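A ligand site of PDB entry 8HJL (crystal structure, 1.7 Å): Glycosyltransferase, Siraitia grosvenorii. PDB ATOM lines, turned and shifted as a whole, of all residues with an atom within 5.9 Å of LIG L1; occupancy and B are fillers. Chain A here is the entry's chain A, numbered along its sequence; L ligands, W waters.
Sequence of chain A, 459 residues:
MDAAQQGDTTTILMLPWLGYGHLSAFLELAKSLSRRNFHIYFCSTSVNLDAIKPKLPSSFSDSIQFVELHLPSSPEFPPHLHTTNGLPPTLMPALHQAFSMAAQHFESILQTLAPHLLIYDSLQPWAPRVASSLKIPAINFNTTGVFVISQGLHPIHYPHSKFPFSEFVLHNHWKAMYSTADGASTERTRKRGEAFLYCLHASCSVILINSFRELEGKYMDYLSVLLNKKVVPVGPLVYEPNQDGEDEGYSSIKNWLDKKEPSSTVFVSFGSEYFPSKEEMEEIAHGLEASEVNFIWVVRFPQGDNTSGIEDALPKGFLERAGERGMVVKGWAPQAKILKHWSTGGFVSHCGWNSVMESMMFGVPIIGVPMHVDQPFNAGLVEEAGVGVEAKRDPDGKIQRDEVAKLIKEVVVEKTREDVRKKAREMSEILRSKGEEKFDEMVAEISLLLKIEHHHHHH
An oxygen (O1) of LIG L1 lies close to an oxygen (O5) of LG2 L2.
Water W3 lies within hydrogen-bond range of an oxygen (O11) of LIG L1 (2.5 Å) and the guanidinium group of Arg 129 (3.4 Å). Water W6 lies within hydrogen-bond range of NE2 of His 157 (2.7 Å), O of Leu 226 (2.7 Å) and O14 of LIG L1 (3.2 Å).
Residues that only touch LIG L1: Tyr 198 (3.1 Å), Asn 228 (3.3 Å), Ala 195 (3.7 Å), Leu 197 (3.8 Å), Leu 227 (3.8 Å), Glu 194 (3.9 Å) and Ile 156 (3.99 Å). Hydrophobic or aromatic side chains within 4 Å of LIG L1: Ile 156, His 157, Leu 197, Tyr 198 and His 201.
A ring nitrogen (NE2) of His 201 sits at hydrogen-bond distance from an oxygen (O7) of LIG L1, 2.7 Å away. A ring nitrogen (ND1) of His 157 is in hydrogen-bond range of an oxygen (O16) of LIG L1, 2.8 Å away. The backbone carbonyl oxygen of Leu 226 sits at hydrogen-bond distance from an oxygen (O17) of LIG L1, 2.8 Å away. O11 of LIG L1 sits at hydrogen-bond distance from NH1 of Arg 129 (2.9 Å). The backbone carbonyl oxygen of Val 225 lies within hydrogen-bond range of an oxygen (O18) of LIG L1 (3.0 Å).
The guanidinium group (NH1) of Arg 129 lies within hydrogen-bond range of the backbone carbonyl oxygen (O) of Pro 125, at 3.4 Å.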
ATOM      1  N   PRO A 125      16.479  -4.846 -23.983  1.00  0.00           N
ATOM      2  CA  PRO A 125      15.558  -5.907 -23.533  1.00  0.00           C
ATOM      3  C   PRO A 125      15.991  -7.297 -23.981  1.00  0.00           C
ATOM      4  O   PRO A 125      15.696  -8.290 -23.304  1.00  0.00           O
ATOM      5  CB  PRO A 125      14.223  -5.494 -24.160  1.00  0.00           C
ATOM      6  CG  PRO A 125      14.392  -4.057 -24.573  1.00  0.00           C
ATOM      7  CD  PRO A 125      15.830  -3.857 -24.852  1.00  0.00           C
ATOM      8  N   ARG A 129      16.912 -11.733 -22.000  1.00  0.00           N
ATOM      9  CA  ARG A 129      16.353 -12.850 -22.757  1.00  0.00           C
ATOM     10  C   ARG A 129      17.448 -13.827 -23.209  1.00  0.00           C
ATOM     11  O   ARG A 129      17.279 -15.043 -23.095  1.00  0.00           O
ATOM     12  CB  ARG A 129      15.581 -12.317 -23.970  1.00  0.00           C
ATOM     13  CG  ARG A 129      14.805 -13.366 -24.714  1.00  0.00           C
ATOM     14  CD  ARG A 129      13.641 -12.753 -25.464  1.00  0.00           C
ATOM     15  NE  ARG A 129      14.063 -11.912 -26.581  1.00  0.00           N
ATOM     16  CZ  ARG A 129      14.080 -10.580 -26.563  1.00  0.00           C
ATOM     17  NH1 ARG A 129      13.716  -9.902 -25.489  1.00  0.00           N
ATOM     18  NH2 ARG A 129      14.470  -9.920 -27.648  1.00  0.00           N
ATOM     19  N   LEU A 153       6.742   5.836 -13.925  1.00  0.00           N
ATOM     20  CA  LEU A 153       5.872   4.688 -13.661  1.00  0.00           C
ATOM     21  C   LEU A 153       4.612   5.091 -12.903  1.00  0.00           C
ATOM     22  O   LEU A 153       3.559   4.478 -13.109  1.00  0.00           O
ATOM     23  CB  LEU A 153       6.669   3.619 -12.898  1.00  0.00           C
ATOM     24  CG  LEU A 153       6.066   2.216 -12.778  1.00  0.00           C
ATOM     25  CD1 LEU A 153       5.525   1.653 -14.117  1.00  0.00           C
ATOM     26  CD2 LEU A 153       7.122   1.293 -12.188  1.00  0.00           C
ATOM     27  N   ILE A 156       1.233   5.589 -14.850  1.00  0.00           N
ATOM     28  CA  ILE A 156       0.684   4.371 -15.410  1.00  0.00           C
ATOM     29  C   ILE A 156      -0.312   3.742 -14.455  1.00  0.00           C
ATOM     30  O   ILE A 156      -1.354   3.226 -14.879  1.00  0.00           O
ATOM     31  CB  ILE A 156       1.829   3.392 -15.751  1.00  0.00           C
ATOM     32  CG1 ILE A 156       2.755   4.020 -16.807  1.00  0.00           C
ATOM     33  CG2 ILE A 156       1.273   2.039 -16.171  1.00  0.00           C
ATOM     34  CD1 ILE A 156       4.038   3.261 -17.044  1.00  0.00           C
ATOM     35  N   HIS A 157      -0.032   3.808 -13.162  1.00  0.00           N
ATOM     36  CA  HIS A 157      -0.912   3.224 -12.161  1.00  0.00           C
ATOM     37  C   HIS A 157      -1.880   4.230 -11.555  1.00  0.00           C
ATOM     38  O   HIS A 157      -2.938   3.837 -11.037  1.00  0.00           O
ATOM     39  CB  HIS A 157      -0.077   2.571 -11.049  1.00  0.00           C
ATOM     40  CG  HIS A 157       0.763   1.431 -11.533  1.00  0.00           C
ATOM     41  ND1 HIS A 157       0.280   0.142 -11.610  1.00  0.00           N
ATOM     42  CD2 HIS A 157       2.037   1.377 -11.982  1.00  0.00           C
ATOM     43  CE1 HIS A 157       1.226  -0.655 -12.071  1.00  0.00           C
ATOM     44  NE2 HIS A 157       2.300   0.071 -12.303  1.00  0.00           N
ATOM     45  N   LYS A 191       5.878   2.241 -26.836  1.00  0.00           N
ATOM     46  CA  LYS A 191       6.775   1.126 -27.124  1.00  0.00           C
ATOM     47  C   LYS A 191       8.157   1.349 -26.498  1.00  0.00           C
ATOM     48  O   LYS A 191       8.763   0.401 -25.977  1.00  0.00           O
ATOM     49  CB  LYS A 191       6.891   0.932 -28.645  1.00  0.00           C
ATOM     50  CG  LYS A 191       5.662   0.284 -29.320  1.00  0.00           C
ATOM     51  CD  LYS A 191       5.849   0.290 -30.830  1.00  0.00           C
ATOM     52  CE  LYS A 191       4.877  -0.617 -31.569  1.00  0.00           C
ATOM     53  NZ  LYS A 191       3.471  -0.119 -31.626  1.00  0.00           N
ATOM     54  N   GLY A 193       8.697   3.072 -23.690  1.00  0.00           N
ATOM     55  CA  GLY A 193       8.505   2.826 -22.269  1.00  0.00           C
ATOM     56  C   GLY A 193       8.339   1.362 -21.932  1.00  0.00           C
ATOM     57  O   GLY A 193       8.792   0.911 -20.864  1.00  0.00           O
ATOM     58  N   GLU A 194       7.727   0.587 -22.827  1.00  0.00           N
ATOM     59  CA  GLU A 194       7.578  -0.838 -22.595  1.00  0.00           C
ATOM     60  C   GLU A 194       8.925  -1.546 -22.601  1.00  0.00           C
ATOM     61  O   GLU A 194       9.162  -2.437 -21.773  1.00  0.00           O
ATOM     62  CB  GLU A 194       6.648  -1.447 -23.642  1.00  0.00           C
ATOM     63  CG  GLU A 194       5.231  -1.054 -23.431  1.00  0.00           C
ATOM     64  CD  GLU A 194       4.335  -1.494 -24.563  1.00  0.00           C
ATOM     65  OE1 GLU A 194       4.852  -2.000 -25.591  1.00  0.00           O
ATOM     66  OE2 GLU A 194       3.111  -1.325 -24.421  1.00  0.00           O
ATOM     67  N   ALA A 195       9.824  -1.149 -23.501  1.00  0.00           N
ATOM     68  CA  ALA A 195      11.116  -1.801 -23.569  1.00  0.00           C
ATOM     69  C   ALA A 195      11.960  -1.452 -22.349  1.00  0.00           C
ATOM     70  O   ALA A 195      12.669  -2.322 -21.807  1.00  0.00           O
ATOM     71  CB  ALA A 195      11.844  -1.399 -24.861  1.00  0.00           C
ATOM     72  N   LEU A 197      10.851  -0.535 -19.295  1.00  0.00           N
ATOM     73  CA  LEU A 197      10.339  -1.185 -18.096  1.00  0.00           C
ATOM     74  C   LEU A 197      10.589  -2.672 -18.122  1.00  0.00           C
ATOM     75  O   LEU A 197      10.798  -3.297 -17.069  1.00  0.00           O
ATOM     76  CB  LEU A 197       8.843  -0.910 -17.964  1.00  0.00           C
ATOM     77  CG  LEU A 197       8.497   0.516 -17.552  1.00  0.00           C
ATOM     78  CD1 LEU A 197       6.979   0.616 -17.356  1.00  0.00           C
ATOM     79  CD2 LEU A 197       9.214   0.935 -16.279  1.00  0.00           C
ATOM     80  N   TYR A 198      10.515  -3.293 -19.313  1.00  0.00           N
ATOM     81  CA  TYR A 198      10.848  -4.700 -19.407  1.00  0.00           C
ATOM     82  C   TYR A 198      12.221  -4.982 -18.810  1.00  0.00           C
ATOM     83  O   TYR A 198      12.396  -5.958 -18.066  1.00  0.00           O
ATOM     84  CB  TYR A 198      10.792  -5.186 -20.861  1.00  0.00           C
ATOM     85  CG  TYR A 198      11.131  -6.660 -20.916  1.00  0.00           C
ATOM     86  CD1 TYR A 198      10.250  -7.610 -20.428  1.00  0.00           C
ATOM     87  CD2 TYR A 198      12.372  -7.087 -21.342  1.00  0.00           C
ATOM     88  CE1 TYR A 198      10.564  -8.942 -20.430  1.00  0.00           C
ATOM     89  CE2 TYR A 198      12.707  -8.426 -21.346  1.00  0.00           C
ATOM     90  CZ  TYR A 198      11.793  -9.344 -20.893  1.00  0.00           C
ATOM     91  OH  TYR A 198      12.108 -10.679 -20.875  1.00  0.00           O
ATOM     92  N   HIS A 201      11.674  -4.985 -15.119  1.00  0.00           N
ATOM     93  CA  HIS A 201      10.752  -6.031 -14.696  1.00  0.00           C
ATOM     94  C   HIS A 201      11.354  -7.417 -14.872  1.00  0.00           C
ATOM     95  O   HIS A 201      11.100  -8.317 -14.050  1.00  0.00           O
ATOM     96  CB  HIS A 201       9.452  -5.862 -15.494  1.00  0.00           C
ATOM     97  CG  HIS A 201       8.513  -7.028 -15.414  1.00  0.00           C
ATOM     98  ND1 HIS A 201       7.645  -7.232 -14.363  1.00  0.00           N
ATOM     99  CD2 HIS A 201       8.244  -8.011 -16.316  1.00  0.00           C
ATOM    100  CE1 HIS A 201       6.910  -8.308 -14.595  1.00  0.00           C
ATOM    101  NE2 HIS A 201       7.266  -8.807 -15.772  1.00  0.00           N
ATOM    102  N   VAL A 225       7.229  -0.676  -4.684  1.00  0.00           N
ATOM    103  CA  VAL A 225       5.820  -1.057  -4.657  1.00  0.00           C
ATOM    104  C   VAL A 225       5.256  -1.082  -6.071  1.00  0.00           C
ATOM    105  O   VAL A 225       4.548  -2.030  -6.446  1.00  0.00           O
ATOM    106  CB  VAL A 225       5.018  -0.113  -3.748  1.00  0.00           C
ATOM    107  CG1 VAL A 225       3.554  -0.439  -3.843  1.00  0.00           C
ATOM    108  CG2 VAL A 225       5.487  -0.236  -2.295  1.00  0.00           C
ATOM    109  N   LEU A 226       5.538  -0.059  -6.885  1.00  0.00           N
ATOM    110  CA  LEU A 226       4.952   0.024  -8.221  1.00  0.00           C
ATOM    111  C   LEU A 226       5.451  -1.105  -9.125  1.00  0.00           C
ATOM    112  O   LEU A 226       4.670  -1.708  -9.859  1.00  0.00           O
ATOM    113  CB  LEU A 226       5.261   1.377  -8.851  1.00  0.00           C
ATOM    114  CG  LEU A 226       4.671   2.618  -8.203  1.00  0.00           C
ATOM    115  CD1 LEU A 226       5.350   3.885  -8.759  1.00  0.00           C
ATOM    116  CD2 LEU A 226       3.169   2.673  -8.419  1.00  0.00           C
ATOM    117  N   LEU A 227       6.755  -1.383  -9.104  1.00  0.00           N
ATOM    118  CA  LEU A 227       7.291  -2.483  -9.912  1.00  0.00           C
ATOM    119  C   LEU A 227       7.054  -3.847  -9.294  1.00  0.00           C
ATOM    120  O   LEU A 227       7.238  -4.856  -9.993  1.00  0.00           O
ATOM    121  CB  LEU A 227       8.792  -2.307 -10.125  1.00  0.00           C
ATOM    122  CG  LEU A 227       9.293  -1.453 -11.271  1.00  0.00           C
ATOM    123  CD1 LEU A 227      10.788  -1.622 -11.366  1.00  0.00           C
ATOM    124  CD2 LEU A 227       8.628  -1.883 -12.567  1.00  0.00           C
ATOM    125  N   ASN A 228       6.654  -3.916  -8.025  1.00  0.00           N
ATOM    126  CA  ASN A 228       6.586  -5.171  -7.281  1.00  0.00           C
ATOM    127  C   ASN A 228       7.920  -5.939  -7.368  1.00  0.00           C
ATOM    128  O   ASN A 228       7.951  -7.142  -7.589  1.00  0.00           O
ATOM    129  CB  ASN A 228       5.417  -6.025  -7.777  1.00  0.00           C
ATOM    130  CG  ASN A 228       5.163  -7.231  -6.881  1.00  0.00           C
ATOM    131  OD1 ASN A 228       4.995  -8.341  -7.369  1.00  0.00           O
ATOM    132  ND2 ASN A 228       5.165  -7.001  -5.579  1.00  0.00           N
HETATM  133  C1  LIG L   1       3.249  -1.410 -16.457  1.00  0.00           C
HETATM  134  C2  LIG L   1       3.596  -2.955 -16.503  1.00  0.00           C
HETATM  135  C3  LIG L   1       5.162  -3.028 -16.716  1.00  0.00           C
HETATM  136  C4  LIG L   1       5.718  -4.128 -17.696  1.00  0.00           C
HETATM  137  C5  LIG L   1       5.472  -5.600 -17.238  1.00  0.00           C
HETATM  138  C6  LIG L   1       4.963  -4.358 -19.030  1.00  0.00           C
HETATM  139  C7  LIG L   1       3.555  -3.648 -19.012  1.00  0.00           C
HETATM  140  C8  LIG L   1       2.821  -3.604 -17.650  1.00  0.00           C
HETATM  141  C9  LIG L   1       5.370  -2.903 -19.341  1.00  0.00           C
HETATM  142  C10 LIG L   1       6.021  -4.546 -20.115  1.00  0.00           C
HETATM  143  C11 LIG L   1       7.236  -5.165 -19.357  1.00  0.00           C
HETATM  144  C12 LIG L   1       7.217  -4.429 -17.985  1.00  0.00           C
HETATM  145  C13 LIG L   1       5.658  -5.493 -21.233  1.00  0.00           C
HETATM  146  C14 LIG L   1       6.972  -6.143 -21.817  1.00  0.00           C
HETATM  147  C15 LIG L   1       7.452  -5.757 -23.291  1.00  0.00           C
HETATM  148  C16 LIG L   1       8.520  -6.767 -23.747  1.00  0.00           C
HETATM  149  C17 LIG L   1       8.671  -9.174 -23.745  1.00  0.00           C
HETATM  150  C18 LIG L   1       7.972 -10.254 -22.844  1.00  0.00           C
HETATM  151  C19 LIG L   1       6.592 -10.191 -20.985  1.00  0.00           C
HETATM  152  C20 LIG L   1       4.275  -9.563 -20.524  1.00  0.00           C
HETATM  153  C21 LIG L   1       3.222  -8.464 -20.935  1.00  0.00           C
HETATM  154  C22 LIG L   1       4.477  -9.633 -18.998  1.00  0.00           C
HETATM  155  C23 LIG L   1       5.605 -10.669 -18.679  1.00  0.00           C
HETATM  156  C24 LIG L   1       6.914 -10.354 -19.506  1.00  0.00           C
HETATM  157  C25 LIG L   1       8.933 -11.426 -22.605  1.00  0.00           C
HETATM  158  C26 LIG L   1       9.887 -11.669 -23.860  1.00  0.00           C
HETATM  159  C27 LIG L   1       9.361 -11.084 -25.179  1.00  0.00           C
HETATM  160  C28 LIG L   1      10.431 -11.189 -26.271  1.00  0.00           C
HETATM  161  C29 LIG L   1       9.209  -6.273 -25.003  1.00  0.00           C
HETATM  162  C30 LIG L   1       8.279  -6.374 -26.172  1.00  0.00           C
HETATM  163  C31 LIG L   1      10.491  -7.021 -25.309  1.00  0.00           C
HETATM  164  C32 LIG L   1       4.905  -4.752 -22.342  1.00  0.00           C
HETATM  165  C33 LIG L   1       5.911  -3.132 -15.395  1.00  0.00           C
HETATM  166  C34 LIG L   1       5.428  -4.173 -14.339  1.00  0.00           C
HETATM  167  C35 LIG L   1       3.943  -4.592 -14.509  1.00  0.00           C
HETATM  168  C36 LIG L   1       3.123  -3.412 -15.021  1.00  0.00           C
HETATM  169  C37 LIG L   1       1.550  -3.565 -14.996  1.00  0.00           C
HETATM  170  C38 LIG L   1       0.959  -4.519 -13.985  1.00  0.00           C
HETATM  171  C39 LIG L   1       1.937  -4.992 -12.887  1.00  0.00           C
HETATM  172  C40 LIG L   1       3.295  -5.483 -13.477  1.00  0.00           C
HETATM  173  C41 LIG L   1       3.107  -6.885 -14.122  1.00  0.00           C
HETATM  174  C42 LIG L   1       4.270  -5.634 -12.298  1.00  0.00           C
HETATM  175  C43 LIG L   1       1.323  -4.064 -10.860  1.00  0.00           C
HETATM  176  C44 LIG L   1      -0.862  -3.460 -10.040  1.00  0.00           C
HETATM  177  C45 LIG L   1      -2.147  -2.652 -10.494  1.00  0.00           C
HETATM  178  C46 LIG L   1      -0.325  -2.850  -8.735  1.00  0.00           C
HETATM  179  C47 LIG L   1       1.184  -3.182  -8.441  1.00  0.00           C
HETATM  180  C48 LIG L   1       2.069  -3.333  -9.741  1.00  0.00           C
HETATM  181  O1  LIG L   1       1.567  -2.919 -17.952  1.00  0.00           O
HETATM  182  O2  LIG L   1       7.864  -8.039 -23.910  1.00  0.00           O
HETATM  183  O3  LIG L   1       7.752  -9.711 -21.601  1.00  0.00           O
HETATM  184  O4  LIG L   1       5.511  -9.224 -21.224  1.00  0.00           O
HETATM  185  O5  LIG L   1       3.062  -8.615 -22.323  1.00  0.00           O
HETATM  186  O6  LIG L   1       7.835 -11.425 -19.352  1.00  0.00           O
HETATM  187  O7  LIG L   1       5.916 -10.614 -17.227  1.00  0.00           O
HETATM  188  O8  LIG L   1       3.317 -10.111 -18.331  1.00  0.00           O
HETATM  189  O9  LIG L   1       8.158 -12.620 -22.309  1.00  0.00           O
HETATM  190  O10 LIG L   1       8.993  -9.623 -25.004  1.00  0.00           O
HETATM  191  O11 LIG L   1      11.024  -9.971 -26.511  1.00  0.00           O
HETATM  192  O12 LIG L   1      10.050 -13.081 -24.025  1.00  0.00           O
HETATM  193  O13 LIG L   1       9.619  -4.961 -24.871  1.00  0.00           O
HETATM  194  O14 LIG L   1       2.163  -3.976 -12.031  1.00  0.00           O
HETATM  195  O15 LIG L   1       0.105  -3.439 -11.152  1.00  0.00           O
HETATM  196  O16 LIG L   1      -1.889  -1.309 -10.710  1.00  0.00           O
HETATM  197  O17 LIG L   1       3.238  -4.072  -9.406  1.00  0.00           O
HETATM  198  O18 LIG L   1       1.749  -2.131  -7.653  1.00  0.00           O
HETATM  199  O19 LIG L   1      -1.122  -3.366  -7.663  1.00  0.00           O
HETATM  200  O1  LG2 L   2      -0.960  -7.536 -16.323  1.00  0.00           O
HETATM  201  O2  LG2 L   2      -3.641  -1.874 -13.512  1.00  0.00           O
HETATM  202  C1  LG2 L   2      -3.024  -0.692 -13.960  1.00  0.00           C
HETATM  203  C2  LG2 L   2      -2.338  -0.969 -15.298  1.00  0.00           C
HETATM  204  O3  LG2 L   2      -2.710  -2.251 -15.729  1.00  0.00           O
HETATM  205  C3  LG2 L   2      -2.240  -2.676 -16.977  1.00  0.00           C
HETATM  206  C4  LG2 L   2      -2.906  -4.032 -17.254  1.00  0.00           C
HETATM  207  O4  LG2 L   2      -2.497  -4.657 -18.441  1.00  0.00           O
HETATM  208  C5  LG2 L   2      -1.309  -4.255 -19.060  1.00  0.00           C
HETATM  209  C6  LG2 L   2      -0.587  -5.516 -19.562  1.00  0.00           C
HETATM  210  O5  LG2 L   2       0.498  -5.843 -18.736  1.00  0.00           O
HETATM  211  C7  LG2 L   2       0.259  -5.720 -17.367  1.00  0.00           C
HETATM  212  C8  LG2 L   2       1.141  -7.997 -17.525  1.00  0.00           C
HETATM  213  C9  LG2 L   2      -0.068  -5.326 -20.996  1.00  0.00           C
HETATM  214  C10 LG2 L   2      -4.413  -3.836 -17.337  1.00  0.00           C
HETATM  215  C11 LG2 L   2      -0.827  -0.903 -15.073  1.00  0.00           C
HETATM  216  O1  LG3 L   3       0.744  -0.114 -20.748  1.00  0.00           O
HETATM  217  C1  LG3 L   3       0.997   0.723 -19.647  1.00  0.00           C
HETATM  218  C2  LG3 L   3       0.271   2.056 -19.852  1.00  0.00           C
HETATM  219  O2  LG3 L   3       2.963   1.503 -20.741  1.00  0.00           O
HETATM  220  C3  LG3 L   3       4.208   2.118 -20.619  1.00  0.00           C
HETATM  221  O3  LG3 L   3       5.910  13.976 -15.462  1.00  0.00           O
HETATM  222  C4  LG3 L   3       6.590  12.797 -15.110  1.00  0.00           C
HETATM  223  C5  LG3 L   3       6.572  11.823 -16.286  1.00  0.00           C
HETATM  224  C6  LG3 L   3       8.016  10.916 -17.915  1.00  0.00           C
HETATM  225  C7  LG3 L   3       9.420  10.343 -17.709  1.00  0.00           C
HETATM  226  O4  LG3 L   3       9.491   9.061 -18.237  1.00  0.00           O
HETATM  227  C8  LG3 L   3      10.772   8.508 -18.106  1.00  0.00           C
HETATM  228  C9  LG3 L   3      10.723   6.987 -18.043  1.00  0.00           C
HETATM  229  O5  LG3 L   3       9.446   6.581 -17.646  1.00  0.00           O
HETATM  230  C10 LG3 L   3       8.622   6.220 -18.716  1.00  0.00           C
HETATM  231  C11 LG3 L   3       8.184   4.778 -18.564  1.00  0.00           C
HETATM  232  O6  LG3 L   3       6.870   4.667 -19.022  1.00  0.00           O
HETATM  233  C12 LG3 L   3       6.646   5.346 -20.228  1.00  0.00           C
HETATM  234  C13 LG3 L   3       5.315   4.910 -20.828  1.00  0.00           C
HETATM  235  C14 LG3 L   3       4.490   2.957 -21.866  1.00  0.00           C
HETATM  236  C15 LG3 L   3       5.280   1.044 -20.477  1.00  0.00           C
HETATM  237  C16 LG3 L   3       4.739   6.070 -21.640  1.00  0.00           C
HETATM  238  C17 LG3 L   3       8.287   4.392 -17.098  1.00  0.00           C
HETATM  239  C18 LG3 L   3      11.774   6.497 -17.049  1.00  0.00           C
HETATM  240  C19 LG3 L   3       9.766  10.244 -16.230  1.00  0.00           C
HETATM  241  C20 LG3 L   3       5.409  12.130 -17.226  1.00  0.00           C
HETATM  242  O   HOH W   1      11.083 -14.430 -22.317  1.00  0.00           O
HETATM  243  O   HOH W   2      10.072 -14.713 -26.349  1.00  0.00           O
HETATM  244  O   HOH W   3      11.397  -9.094 -28.776  1.00  0.00           O
HETATM  245  O   HOH W   4       4.967  -8.292 -24.290  1.00  0.00           O
HETATM  246  O   HOH W   5       2.510 -12.890 -18.133  1.00  0.00           O
HETATM  247  O   HOH W   6       4.312  -1.639 -12.557  1.00  0.00           O
HETATM  248  O   HOH W   7       6.619 -13.654 -18.587  1.00  0.00           O
HETATM  249  O   HOH W   8       3.812 -10.168 -15.106  1.00  0.00           O
HETATM  250  O   HOH W   9      12.266  -6.876 -27.838  1.00  0.00           O
